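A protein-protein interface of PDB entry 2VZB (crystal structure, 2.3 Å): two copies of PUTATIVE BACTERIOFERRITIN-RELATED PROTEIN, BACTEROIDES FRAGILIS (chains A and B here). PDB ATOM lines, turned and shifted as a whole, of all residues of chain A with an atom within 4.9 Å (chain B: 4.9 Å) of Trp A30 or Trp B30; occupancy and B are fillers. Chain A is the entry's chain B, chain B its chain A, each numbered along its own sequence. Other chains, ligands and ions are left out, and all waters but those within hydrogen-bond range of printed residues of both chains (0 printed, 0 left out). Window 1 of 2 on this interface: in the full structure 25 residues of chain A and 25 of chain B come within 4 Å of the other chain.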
ATOM      1  N   LEU A  26       2.064  -6.716 -31.437  1.00  0.00           N
ATOM      2  CA  LEU A  26       3.332  -6.121 -30.989  1.00  0.00           C
ATOM      3  C   LEU A  26       3.205  -5.580 -29.564  1.00  0.00           C
ATOM      4  O   LEU A  26       4.028  -5.861 -28.674  1.00  0.00           O
ATOM      5  CB  LEU A  26       3.754  -5.016 -31.954  1.00  0.00           C
ATOM      6  CG  LEU A  26       5.074  -4.278 -31.687  1.00  0.00           C
ATOM      7  CD1 LEU A  26       6.220  -5.275 -31.463  1.00  0.00           C
ATOM      8  CD2 LEU A  26       5.392  -3.335 -32.848  1.00  0.00           C
ATOM      9  N   SER A  27       2.139  -4.826 -29.353  1.00  0.00           N
ATOM     10  CA  SER A  27       1.814  -4.275 -28.051  1.00  0.00           C
ATOM     11  C   SER A  27       1.734  -5.369 -27.003  1.00  0.00           C
ATOM     12  O   SER A  27       2.288  -5.262 -25.921  1.00  0.00           O
ATOM     13  CB  SER A  27       0.498  -3.512 -28.140  1.00  0.00           C
ATOM     14  OG  SER A  27       0.595  -2.440 -29.076  1.00  0.00           O
ATOM     15  N   GLU A  28       1.034  -6.431 -27.358  1.00  0.00           N
ATOM     16  CA  GLU A  28       0.850  -7.581 -26.499  1.00  0.00           C
ATOM     17  C   GLU A  28       2.170  -8.296 -26.161  1.00  0.00           C
ATOM     18  O   GLU A  28       2.382  -8.732 -25.024  1.00  0.00           O
ATOM     19  CB  GLU A  28      -0.132  -8.553 -27.170  1.00  0.00           C
ATOM     20  CG  GLU A  28      -1.580  -8.043 -27.138  1.00  0.00           C
ATOM     21  CD  GLU A  28      -2.528  -8.761 -28.080  1.00  0.00           C
ATOM     22  OE1 GLU A  28      -2.084  -9.606 -28.885  1.00  0.00           O
ATOM     23  OE2 GLU A  28      -3.738  -8.473 -28.005  1.00  0.00           O
ATOM     24  N   GLU A  29       3.043  -8.434 -27.153  1.00  0.00           N
ATOM     25  CA  GLU A  29       4.373  -9.039 -26.941  1.00  0.00           C
ATOM     26  C   GLU A  29       5.204  -8.251 -25.924  1.00  0.00           C
ATOM     27  O   GLU A  29       5.809  -8.830 -25.043  1.00  0.00           O
ATOM     28  CB  GLU A  29       5.145  -9.156 -28.256  1.00  0.00           C
ATOM     29  CG  GLU A  29       4.567 -10.159 -29.209  1.00  0.00           C
ATOM     30  CD  GLU A  29       4.687 -11.567 -28.716  1.00  0.00           C
ATOM     31  OE1 GLU A  29       5.461 -11.815 -27.770  1.00  0.00           O
ATOM     32  OE2 GLU A  29       4.006 -12.438 -29.283  1.00  0.00           O
ATOM     33  N   TRP A  30       5.227  -6.935 -26.047  1.00  0.00           N
ATOM     34  CA  TRP A  30       5.970  -6.096 -25.097  1.00  0.00           C
ATOM     35  C   TRP A  30       5.437  -6.199 -23.672  1.00  0.00           C
ATOM     36  O   TRP A  30       6.218  -6.212 -22.704  1.00  0.00           O
ATOM     37  CB  TRP A  30       6.035  -4.642 -25.555  1.00  0.00           C
ATOM     38  CG  TRP A  30       7.158  -4.440 -26.516  1.00  0.00           C
ATOM     39  CD1 TRP A  30       7.106  -4.557 -27.875  1.00  0.00           C
ATOM     40  CD2 TRP A  30       8.526  -4.146 -26.188  1.00  0.00           C
ATOM     41  NE1 TRP A  30       8.356  -4.341 -28.417  1.00  0.00           N
ATOM     42  CE2 TRP A  30       9.243  -4.092 -27.397  1.00  0.00           C
ATOM     43  CE3 TRP A  30       9.208  -3.911 -24.988  1.00  0.00           C
ATOM     44  CZ2 TRP A  30      10.600  -3.784 -27.445  1.00  0.00           C
ATOM     45  CZ3 TRP A  30      10.559  -3.625 -25.033  1.00  0.00           C
ATOM     46  CH2 TRP A  30      11.241  -3.561 -26.256  1.00  0.00           C
ATOM     47  N   LEU A  31       4.122  -6.310 -23.543  1.00  0.00           N
ATOM     48  CA  LEU A  31       3.500  -6.465 -22.243  1.00  0.00           C
ATOM     49  C   LEU A  31       3.813  -7.851 -21.663  1.00  0.00           C
ATOM     50  O   LEU A  31       4.183  -7.981 -20.493  1.00  0.00           O
ATOM     51  CB  LEU A  31       1.983  -6.233 -22.337  1.00  0.00           C
ATOM     52  CG  LEU A  31       1.524  -4.796 -22.678  1.00  0.00           C
ATOM     53  CD1 LEU A  31       0.003  -4.773 -22.911  1.00  0.00           C
ATOM     54  CD2 LEU A  31       1.905  -3.809 -21.596  1.00  0.00           C
ATOM     55  N   ALA A  32       3.656  -8.876 -22.489  1.00  0.00           N
ATOM     56  CA  ALA A  32       3.969 -10.255 -22.086  1.00  0.00           C
ATOM     57  C   ALA A  32       5.453 -10.401 -21.707  1.00  0.00           C
ATOM     58  O   ALA A  32       5.795 -11.061 -20.730  1.00  0.00           O
ATOM     59  CB  ALA A  32       3.603 -11.232 -23.199  1.00  0.00           C
ATOM     60  N   TYR A  33       6.312  -9.757 -22.494  1.00  0.00           N
ATOM     61  CA  TYR A  33       7.752  -9.672 -22.242  1.00  0.00           C
ATOM     62  C   TYR A  33       8.017  -9.127 -20.830  1.00  0.00           C
ATOM     63  O   TYR A  33       8.618  -9.798 -19.995  1.00  0.00           O
ATOM     64  CB  TYR A  33       8.382  -8.814 -23.353  1.00  0.00           C
ATOM     65  CG  TYR A  33       9.844  -8.433 -23.257  1.00  0.00           C
ATOM     66  CD1 TYR A  33      10.777  -9.206 -22.563  1.00  0.00           C
ATOM     67  CD2 TYR A  33      10.304  -7.304 -23.917  1.00  0.00           C
ATOM     68  CE1 TYR A  33      12.116  -8.831 -22.503  1.00  0.00           C
ATOM     69  CE2 TYR A  33      11.630  -6.923 -23.852  1.00  0.00           C
ATOM     70  CZ  TYR A  33      12.537  -7.694 -23.157  1.00  0.00           C
ATOM     71  OH  TYR A  33      13.861  -7.296 -23.140  1.00  0.00           O
ATOM     72  N   TYR A  34       7.530  -7.936 -20.549  1.00  0.00           N
ATOM     73  CA  TYR A  34       7.733  -7.320 -19.233  1.00  0.00           C
ATOM     74  C   TYR A  34       7.124  -8.140 -18.097  1.00  0.00           C
ATOM     75  O   TYR A  34       7.699  -8.275 -17.013  1.00  0.00           O
ATOM     76  CB  TYR A  34       7.144  -5.914 -19.181  1.00  0.00           C
ATOM     77  CG  TYR A  34       7.682  -5.143 -18.009  1.00  0.00           C
ATOM     78  CD1 TYR A  34       8.958  -4.594 -18.053  1.00  0.00           C
ATOM     79  CD2 TYR A  34       6.942  -4.996 -16.836  1.00  0.00           C
ATOM     80  CE1 TYR A  34       9.483  -3.880 -16.976  1.00  0.00           C
ATOM     81  CE2 TYR A  34       7.455  -4.271 -15.744  1.00  0.00           C
ATOM     82  CZ  TYR A  34       8.727  -3.714 -15.835  1.00  0.00           C
ATOM     83  OH  TYR A  34       9.267  -3.009 -14.791  1.00  0.00           O
ATOM     84  N   TRP A  37       9.376 -10.855 -17.343  1.00  0.00           N
ATOM     85  CA  TRP A  37      10.636 -10.308 -16.859  1.00  0.00           C
ATOM     86  C   TRP A  37      10.562  -9.932 -15.378  1.00  0.00           C
ATOM     87  O   TRP A  37      11.470 -10.236 -14.577  1.00  0.00           O
ATOM     88  CB  TRP A  37      11.015  -9.096 -17.714  1.00  0.00           C
ATOM     89  CG  TRP A  37      12.350  -8.516 -17.398  1.00  0.00           C
ATOM     90  CD1 TRP A  37      13.555  -8.938 -17.864  1.00  0.00           C
ATOM     91  CD2 TRP A  37      12.615  -7.388 -16.570  1.00  0.00           C
ATOM     92  NE1 TRP A  37      14.553  -8.144 -17.375  1.00  0.00           N
ATOM     93  CE2 TRP A  37      14.006  -7.193 -16.563  1.00  0.00           C
ATOM     94  CE3 TRP A  37      11.809  -6.524 -15.830  1.00  0.00           C
ATOM     95  CZ2 TRP A  37      14.610  -6.179 -15.850  1.00  0.00           C
ATOM     96  CZ3 TRP A  37      12.413  -5.508 -15.124  1.00  0.00           C
ATOM     97  CH2 TRP A  37      13.793  -5.347 -15.130  1.00  0.00           C
ATOM     98  N   ARG A  63      10.245 -11.195 -26.489  1.00  0.00           N
ATOM     99  CA  ARG A  63      11.046 -10.117 -27.063  1.00  0.00           C
ATOM    100  C   ARG A  63      11.342 -10.429 -28.540  1.00  0.00           C
ATOM    101  O   ARG A  63      11.055  -9.619 -29.418  1.00  0.00           O
ATOM    102  CB  ARG A  63      12.324  -9.915 -26.244  1.00  0.00           C
ATOM    103  CG  ARG A  63      13.386  -9.042 -26.874  1.00  0.00           C
ATOM    104  CD  ARG A  63      13.009  -7.563 -26.994  1.00  0.00           C
ATOM    105  NE  ARG A  63      14.105  -6.875 -27.687  1.00  0.00           N
ATOM    106  CZ  ARG A  63      14.268  -6.874 -29.004  1.00  0.00           C
ATOM    107  NH1 ARG A  63      13.385  -7.464 -29.802  1.00  0.00           N
ATOM    108  NH2 ARG A  63      15.314  -6.272 -29.523  1.00  0.00           N
ATOM    109  N   ALA A  66       8.360  -9.974 -30.758  1.00  0.00           N
ATOM    110  CA  ALA A  66       8.195  -8.523 -31.008  1.00  0.00           C
ATOM    111  C   ALA A  66       9.004  -8.063 -32.235  1.00  0.00           C
ATOM    112  O   ALA A  66       8.499  -7.321 -33.085  1.00  0.00           O
ATOM    113  CB  ALA A  66       8.583  -7.722 -29.775  1.00  0.00           C
ATOM    114  N   TRP A  87       0.447   0.917 -25.988  1.00  0.00           N
ATOM    115  CA  TRP A  87       0.355  -0.554 -25.882  1.00  0.00           C
ATOM    116  C   TRP A  87      -0.979  -0.966 -25.245  1.00  0.00           C
ATOM    117  O   TRP A  87      -1.668  -1.869 -25.712  1.00  0.00           O
ATOM    118  CB  TRP A  87       1.455  -1.170 -25.011  1.00  0.00           C
ATOM    119  CG  TRP A  87       2.852  -1.077 -25.495  1.00  0.00           C
ATOM    120  CD1 TRP A  87       3.292  -0.908 -26.784  1.00  0.00           C
ATOM    121  CD2 TRP A  87       4.020  -1.203 -24.687  1.00  0.00           C
ATOM    122  NE1 TRP A  87       4.662  -0.876 -26.810  1.00  0.00           N
ATOM    123  CE2 TRP A  87       5.132  -1.074 -25.538  1.00  0.00           C
ATOM    124  CE3 TRP A  87       4.232  -1.412 -23.316  1.00  0.00           C
ATOM    125  CZ2 TRP A  87       6.439  -1.141 -25.062  1.00  0.00           C
ATOM    126  CZ3 TRP A  87       5.522  -1.476 -22.844  1.00  0.00           C
ATOM    127  CH2 TRP A  87       6.614  -1.338 -23.715  1.00  0.00           C
ATOM    128  N   LEU B  26      15.204   2.435 -13.344  1.00  0.00           N
ATOM    129  CA  LEU B  26      14.693   1.242 -14.036  1.00  0.00           C
ATOM    130  C   LEU B  26      13.630   1.618 -15.068  1.00  0.00           C
ATOM    131  O   LEU B  26      13.678   1.221 -16.242  1.00  0.00           O
ATOM    132  CB  LEU B  26      14.121   0.241 -13.017  1.00  0.00           C
ATOM    133  CG  LEU B  26      13.549  -1.071 -13.537  1.00  0.00           C
ATOM    134  CD1 LEU B  26      14.565  -1.761 -14.455  1.00  0.00           C
ATOM    135  CD2 LEU B  26      13.143  -1.980 -12.370  1.00  0.00           C
ATOM    136  N   SER B  27      12.675   2.411 -14.610  1.00  0.00           N
ATOM    137  CA  SER B  27      11.622   2.953 -15.479  1.00  0.00           C
ATOM    138  C   SER B  27      12.242   3.666 -16.673  1.00  0.00           C
ATOM    139  O   SER B  27      11.844   3.471 -17.804  1.00  0.00           O
ATOM    140  CB  SER B  27      10.726   3.931 -14.688  1.00  0.00           C
ATOM    141  OG  SER B  27      10.058   3.289 -13.600  1.00  0.00           O
ATOM    142  N   GLU B  28      13.221   4.507 -16.400  1.00  0.00           N
ATOM    143  CA  GLU B  28      13.915   5.262 -17.452  1.00  0.00           C
ATOM    144  C   GLU B  28      14.633   4.370 -18.468  1.00  0.00           C
ATOM    145  O   GLU B  28      14.635   4.667 -19.662  1.00  0.00           O
ATOM    146  CB  GLU B  28      14.908   6.242 -16.808  1.00  0.00           C
ATOM    147  CG  GLU B  28      14.196   7.387 -16.138  1.00  0.00           C
ATOM    148  CD  GLU B  28      15.052   8.144 -15.172  1.00  0.00           C
ATOM    149  OE1 GLU B  28      16.207   7.734 -14.959  1.00  0.00           O
ATOM    150  OE2 GLU B  28      14.564   9.162 -14.633  1.00  0.00           O
ATOM    151  N   GLU B  29      15.252   3.293 -17.980  1.00  0.00           N
ATOM    152  CA  GLU B  29      15.962   2.336 -18.848  1.00  0.00           C
ATOM    153  C   GLU B  29      14.997   1.689 -19.840  1.00  0.00           C
ATOM    154  O   GLU B  29      15.276   1.610 -21.016  1.00  0.00           O
ATOM    155  CB  GLU B  29      16.687   1.264 -18.015  1.00  0.00           C
ATOM    156  CG  GLU B  29      17.910   1.792 -17.243  1.00  0.00           C
ATOM    157  CD  GLU B  29      19.026   2.255 -18.158  1.00  0.00           C
ATOM    158  OE1 GLU B  29      19.028   1.882 -19.359  1.00  0.00           O
ATOM    159  OE2 GLU B  29      19.920   3.005 -17.679  1.00  0.00           O
ATOM    160  N   TRP B  30      13.849   1.244 -19.353  1.00  0.00           N
ATOM    161  CA  TRP B  30      12.865   0.593 -20.210  1.00  0.00           C
ATOM    162  C   TRP B  30      12.334   1.529 -21.274  1.00  0.00           C
ATOM    163  O   TRP B  30      12.084   1.110 -22.420  1.00  0.00           O
ATOM    164  CB  TRP B  30      11.729  -0.017 -19.395  1.00  0.00           C
ATOM    165  CG  TRP B  30      12.086  -1.398 -18.918  1.00  0.00           C
ATOM    166  CD1 TRP B  30      12.677  -1.723 -17.743  1.00  0.00           C
ATOM    167  CD2 TRP B  30      11.898  -2.626 -19.628  1.00  0.00           C
ATOM    168  NE1 TRP B  30      12.859  -3.085 -17.660  1.00  0.00           N
ATOM    169  CE2 TRP B  30      12.395  -3.663 -18.811  1.00  0.00           C
ATOM    170  CE3 TRP B  30      11.347  -2.953 -20.880  1.00  0.00           C
ATOM    171  CZ2 TRP B  30      12.362  -4.994 -19.195  1.00  0.00           C
ATOM    172  CZ3 TRP B  30      11.311  -4.278 -21.256  1.00  0.00           C
ATOM    173  CH2 TRP B  30      11.820  -5.284 -20.415  1.00  0.00           C
ATOM    174  N   LEU B  31      12.177   2.797 -20.902  1.00  0.00           N
ATOM    175  CA  LEU B  31      11.713   3.826 -21.858  1.00  0.00           C
ATOM    176  C   LEU B  31      12.808   4.142 -22.900  1.00  0.00           C
ATOM    177  O   LEU B  31      12.539   4.185 -24.099  1.00  0.00           O
ATOM    178  CB  LEU B  31      11.273   5.096 -21.136  1.00  0.00           C
ATOM    179  CG  LEU B  31      10.028   4.990 -20.250  1.00  0.00           C
ATOM    180  CD1 LEU B  31       9.807   6.290 -19.444  1.00  0.00           C
ATOM    181  CD2 LEU B  31       8.777   4.622 -21.061  1.00  0.00           C
ATOM    182  N   ALA B  32      14.034   4.317 -22.422  1.00  0.00           N
ATOM    183  CA  ALA B  32      15.203   4.510 -23.293  1.00  0.00           C
ATOM    184  C   ALA B  32      15.420   3.324 -24.238  1.00  0.00           C
ATOM    185  O   ALA B  32      15.678   3.494 -25.426  1.00  0.00           O
ATOM    186  CB  ALA B  32      16.442   4.776 -22.461  1.00  0.00           C
ATOM    187  N   TYR B  33      15.261   2.129 -23.693  1.00  0.00           N
ATOM    188  CA  TYR B  33      15.325   0.871 -24.448  1.00  0.00           C
ATOM    189  C   TYR B  33      14.334   0.865 -25.606  1.00  0.00           C
ATOM    190  O   TYR B  33      14.711   0.675 -26.765  1.00  0.00           O
ATOM    191  CB  TYR B  33      15.083  -0.296 -23.462  1.00  0.00           C
ATOM    192  CG  TYR B  33      14.924  -1.702 -24.000  1.00  0.00           C
ATOM    193  CD1 TYR B  33      15.540  -2.122 -25.168  1.00  0.00           C
ATOM    194  CD2 TYR B  33      14.219  -2.641 -23.261  1.00  0.00           C
ATOM    195  CE1 TYR B  33      15.392  -3.429 -25.617  1.00  0.00           C
ATOM    196  CE2 TYR B  33      14.077  -3.926 -23.695  1.00  0.00           C
ATOM    197  CZ  TYR B  33      14.662  -4.317 -24.867  1.00  0.00           C
ATOM    198  OH  TYR B  33      14.500  -5.611 -25.252  1.00  0.00           O
ATOM    199  N   TYR B  34      13.065   1.075 -25.300  1.00  0.00           N
ATOM    200  CA  TYR B  34      12.035   1.093 -26.332  1.00  0.00           C
ATOM    201  C   TYR B  34      12.254   2.204 -27.335  1.00  0.00           C
ATOM    202  O   TYR B  34      12.090   2.003 -28.551  1.00  0.00           O
ATOM    203  CB  TYR B  34      10.627   1.237 -25.735  1.00  0.00           C
ATOM    204  CG  TYR B  34       9.562   0.878 -26.736  1.00  0.00           C
ATOM    205  CD1 TYR B  34       9.285  -0.453 -27.023  1.00  0.00           C
ATOM    206  CD2 TYR B  34       8.878   1.855 -27.444  1.00  0.00           C
ATOM    207  CE1 TYR B  34       8.329  -0.801 -27.958  1.00  0.00           C
ATOM    208  CE2 TYR B  34       7.906   1.505 -28.396  1.00  0.00           C
ATOM    209  CZ  TYR B  34       7.641   0.174 -28.635  1.00  0.00           C
ATOM    210  OH  TYR B  34       6.695  -0.206 -29.552  1.00  0.00           O
ATOM    211  N   TRP B  37      14.818   1.181 -29.704  1.00  0.00           N
ATOM    212  CA  TRP B  37      14.347  -0.003 -30.441  1.00  0.00           C
ATOM    213  C   TRP B  37      13.402   0.382 -31.588  1.00  0.00           C
ATOM    214  O   TRP B  37      13.494  -0.135 -32.696  1.00  0.00           O
ATOM    215  CB  TRP B  37      13.643  -0.961 -29.468  1.00  0.00           C
ATOM    216  CG  TRP B  37      13.202  -2.250 -30.064  1.00  0.00           C
ATOM    217  CD1 TRP B  37      13.953  -3.375 -30.234  1.00  0.00           C
ATOM    218  CD2 TRP B  37      11.892  -2.566 -30.553  1.00  0.00           C
ATOM    219  NE1 TRP B  37      13.196  -4.368 -30.810  1.00  0.00           N
ATOM    220  CE2 TRP B  37      11.929  -3.898 -31.012  1.00  0.00           C
ATOM    221  CE3 TRP B  37      10.691  -1.852 -30.648  1.00  0.00           C
ATOM    222  CZ2 TRP B  37      10.821  -4.517 -31.571  1.00  0.00           C
ATOM    223  CZ3 TRP B  37       9.591  -2.473 -31.190  1.00  0.00           C
ATOM    224  CH2 TRP B  37       9.661  -3.786 -31.652  1.00  0.00           C
ATOM    225  N   ARG B  63      18.784  -2.287 -22.196  1.00  0.00           N
ATOM    226  CA  ARG B  63      18.167  -3.527 -21.731  1.00  0.00           C
ATOM    227  C   ARG B  63      18.984  -4.200 -20.631  1.00  0.00           C
ATOM    228  O   ARG B  63      18.413  -4.637 -19.637  1.00  0.00           O
ATOM    229  CB  ARG B  63      17.978  -4.482 -22.893  1.00  0.00           C
ATOM    230  CG  ARG B  63      17.342  -5.824 -22.544  1.00  0.00           C
ATOM    231  CD  ARG B  63      16.096  -5.742 -21.679  1.00  0.00           C
ATOM    232  NE  ARG B  63      15.641  -7.108 -21.384  1.00  0.00           N
ATOM    233  CZ  ARG B  63      16.054  -7.838 -20.354  1.00  0.00           C
ATOM    234  NH1 ARG B  63      16.927  -7.352 -19.456  1.00  0.00           N
ATOM    235  NH2 ARG B  63      15.573  -9.069 -20.224  1.00  0.00           N
ATOM    236  N   ALA B  66      18.921  -2.151 -17.313  1.00  0.00           N
ATOM    237  CA  ALA B  66      17.679  -2.493 -16.602  1.00  0.00           C
ATOM    238  C   ALA B  66      17.842  -3.717 -15.695  1.00  0.00           C
ATOM    239  O   ALA B  66      17.371  -3.719 -14.544  1.00  0.00           O
ATOM    240  CB  ALA B  66      16.544  -2.722 -17.589  1.00  0.00           C
ATOM    241  N   TRP B  87       5.872   3.364 -15.259  1.00  0.00           N
ATOM    242  CA  TRP B  87       7.175   3.884 -15.723  1.00  0.00           C
ATOM    243  C   TRP B  87       7.112   5.407 -15.857  1.00  0.00           C
ATOM    244  O   TRP B  87       7.997   6.138 -15.410  1.00  0.00           O
ATOM    245  CB  TRP B  87       7.589   3.313 -17.089  1.00  0.00           C
ATOM    246  CG  TRP B  87       7.917   1.854 -17.174  1.00  0.00           C
ATOM    247  CD1 TRP B  87       8.312   1.016 -16.164  1.00  0.00           C
ATOM    248  CD2 TRP B  87       7.930   1.074 -18.367  1.00  0.00           C
ATOM    249  NE1 TRP B  87       8.528  -0.249 -16.655  1.00  0.00           N
ATOM    250  CE2 TRP B  87       8.313  -0.239 -18.008  1.00  0.00           C
ATOM    251  CE3 TRP B  87       7.652   1.353 -19.711  1.00  0.00           C
ATOM    252  CZ2 TRP B  87       8.419  -1.271 -18.956  1.00  0.00           C
ATOM    253  CZ3 TRP B  87       7.757   0.330 -20.640  1.00  0.00           C
ATOM    254  CH2 TRP B  87       8.143  -0.965 -20.258  1.00  0.00           C
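The side-chain hydroxyl (OH) of Tyr B33 sits at hydrogen-bond distance from the side-chain hydroxyl (OH) of Tyr A33. The guanidinium group (NE) of Arg A63 is in hydrogen-bond range of the side-chain hydroxyl (OH) of Tyr B33 (2.8 Å). OH of Tyr B34 sits at hydrogen-bond distance from NE1 of Trp A87 (3.5 Å). OH of Tyr A33 lies within hydrogen-bond range of NE of Arg B63 (2.5 Å). NE1 of Trp B87 is in hydrogen-bond range of OH of Tyr A34. The indole nitrogen of Trp A37 sits close to the guanidinium group of Arg B63, 3.2 Å away. The guanidinium group (NH2) of Arg A63 lies close to the indole nitrogen (NE1) of Trp B37, at 3.1 Å.
CH2 of Trp B37 touches CD1 of Leu A26 (3.8 Å). Trp A30 touches Trp B30 (CZ3 to CZ3, 3.9 Å). Trp A30 touches Tyr B33 (CH2 to CZ, 3.8 Å). Trp A30 touches Tyr B34 (CE2 to CE1, 3.5 Å). Trp B37 touches Trp A30. CE2 of Tyr A33 touches CZ3 of Trp B30, at 3.7 Å. Trp B30 touches Trp A37 (NE1 to CH2, 3.5 Å). Ala B66 touches Trp A37. Ala A66 touches Trp B37. Trp A87 touches Trp B87.
Glu A28 touches none of the printed residues of chain B. Trp A30 touches four residues of chain B. Printed residues of chain B within 4 Å of Arg A63: Tyr B33 (2.8 Å) and Trp B37 (3.1 Å). Of the printed residues of chain A, Leu B26 touches Trp A37. Glu B28 touches none of the printed residues of chain A. Of chain A, only Trp A30, Tyr A33, Tyr A34 and Trp A37 come within 4 Å of Trp B30. Printed residues of chain A within 4 Å of Trp B37: Leu A26, Trp A30, Arg A63 and Ala A66. The nearest printed residue of chain B that does not touch Trp A30 is Trp B87 (5.7 Å).
Printed residues of chain B that touch a printed residue of chain A: Leu B26, Trp B30, Tyr B33, Tyr B34, Trp B37, Arg B63, Ala B66 and Trp B87. Hydrophobic or aromatic side chains of chain B within 4 Å of the printed part of chain A: Leu B26, Trp B30, Tyr B33, Tyr B34, Trp B37 and Trp B87. Printed residues of chain A that touch a printed residue of chain B: Leu A26, Trp A30, Tyr A33, Tyr A34, Trp A37, Arg A63, Ala A66 and Trp A87. Hydrophobic or aromatic side chains of chain A within 4 Å of the printed part of chain B: Leu A26, Trp A30, Tyr A33, Tyr A34, Trp A37 and Trp A87. Among the printed residues, 19 pairs touch across the chains. Among the printed residues, no Asp or Glu carboxylate lies within 4 Å of a Lys or Arg side-chain nitrogen of the other chain.
Leu A26 touches Trp B37, and with the chains exchanged Trp A37 touches Leu B26. Trp A30 touches Tyr B34, and with the chains exchanged Tyr A34 touches Trp B30. Tyr A34 touches Trp B87, and with the chains exchanged Trp A87 touches Tyr B34. Trp A87 touches its own counterpart, Trp B87.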
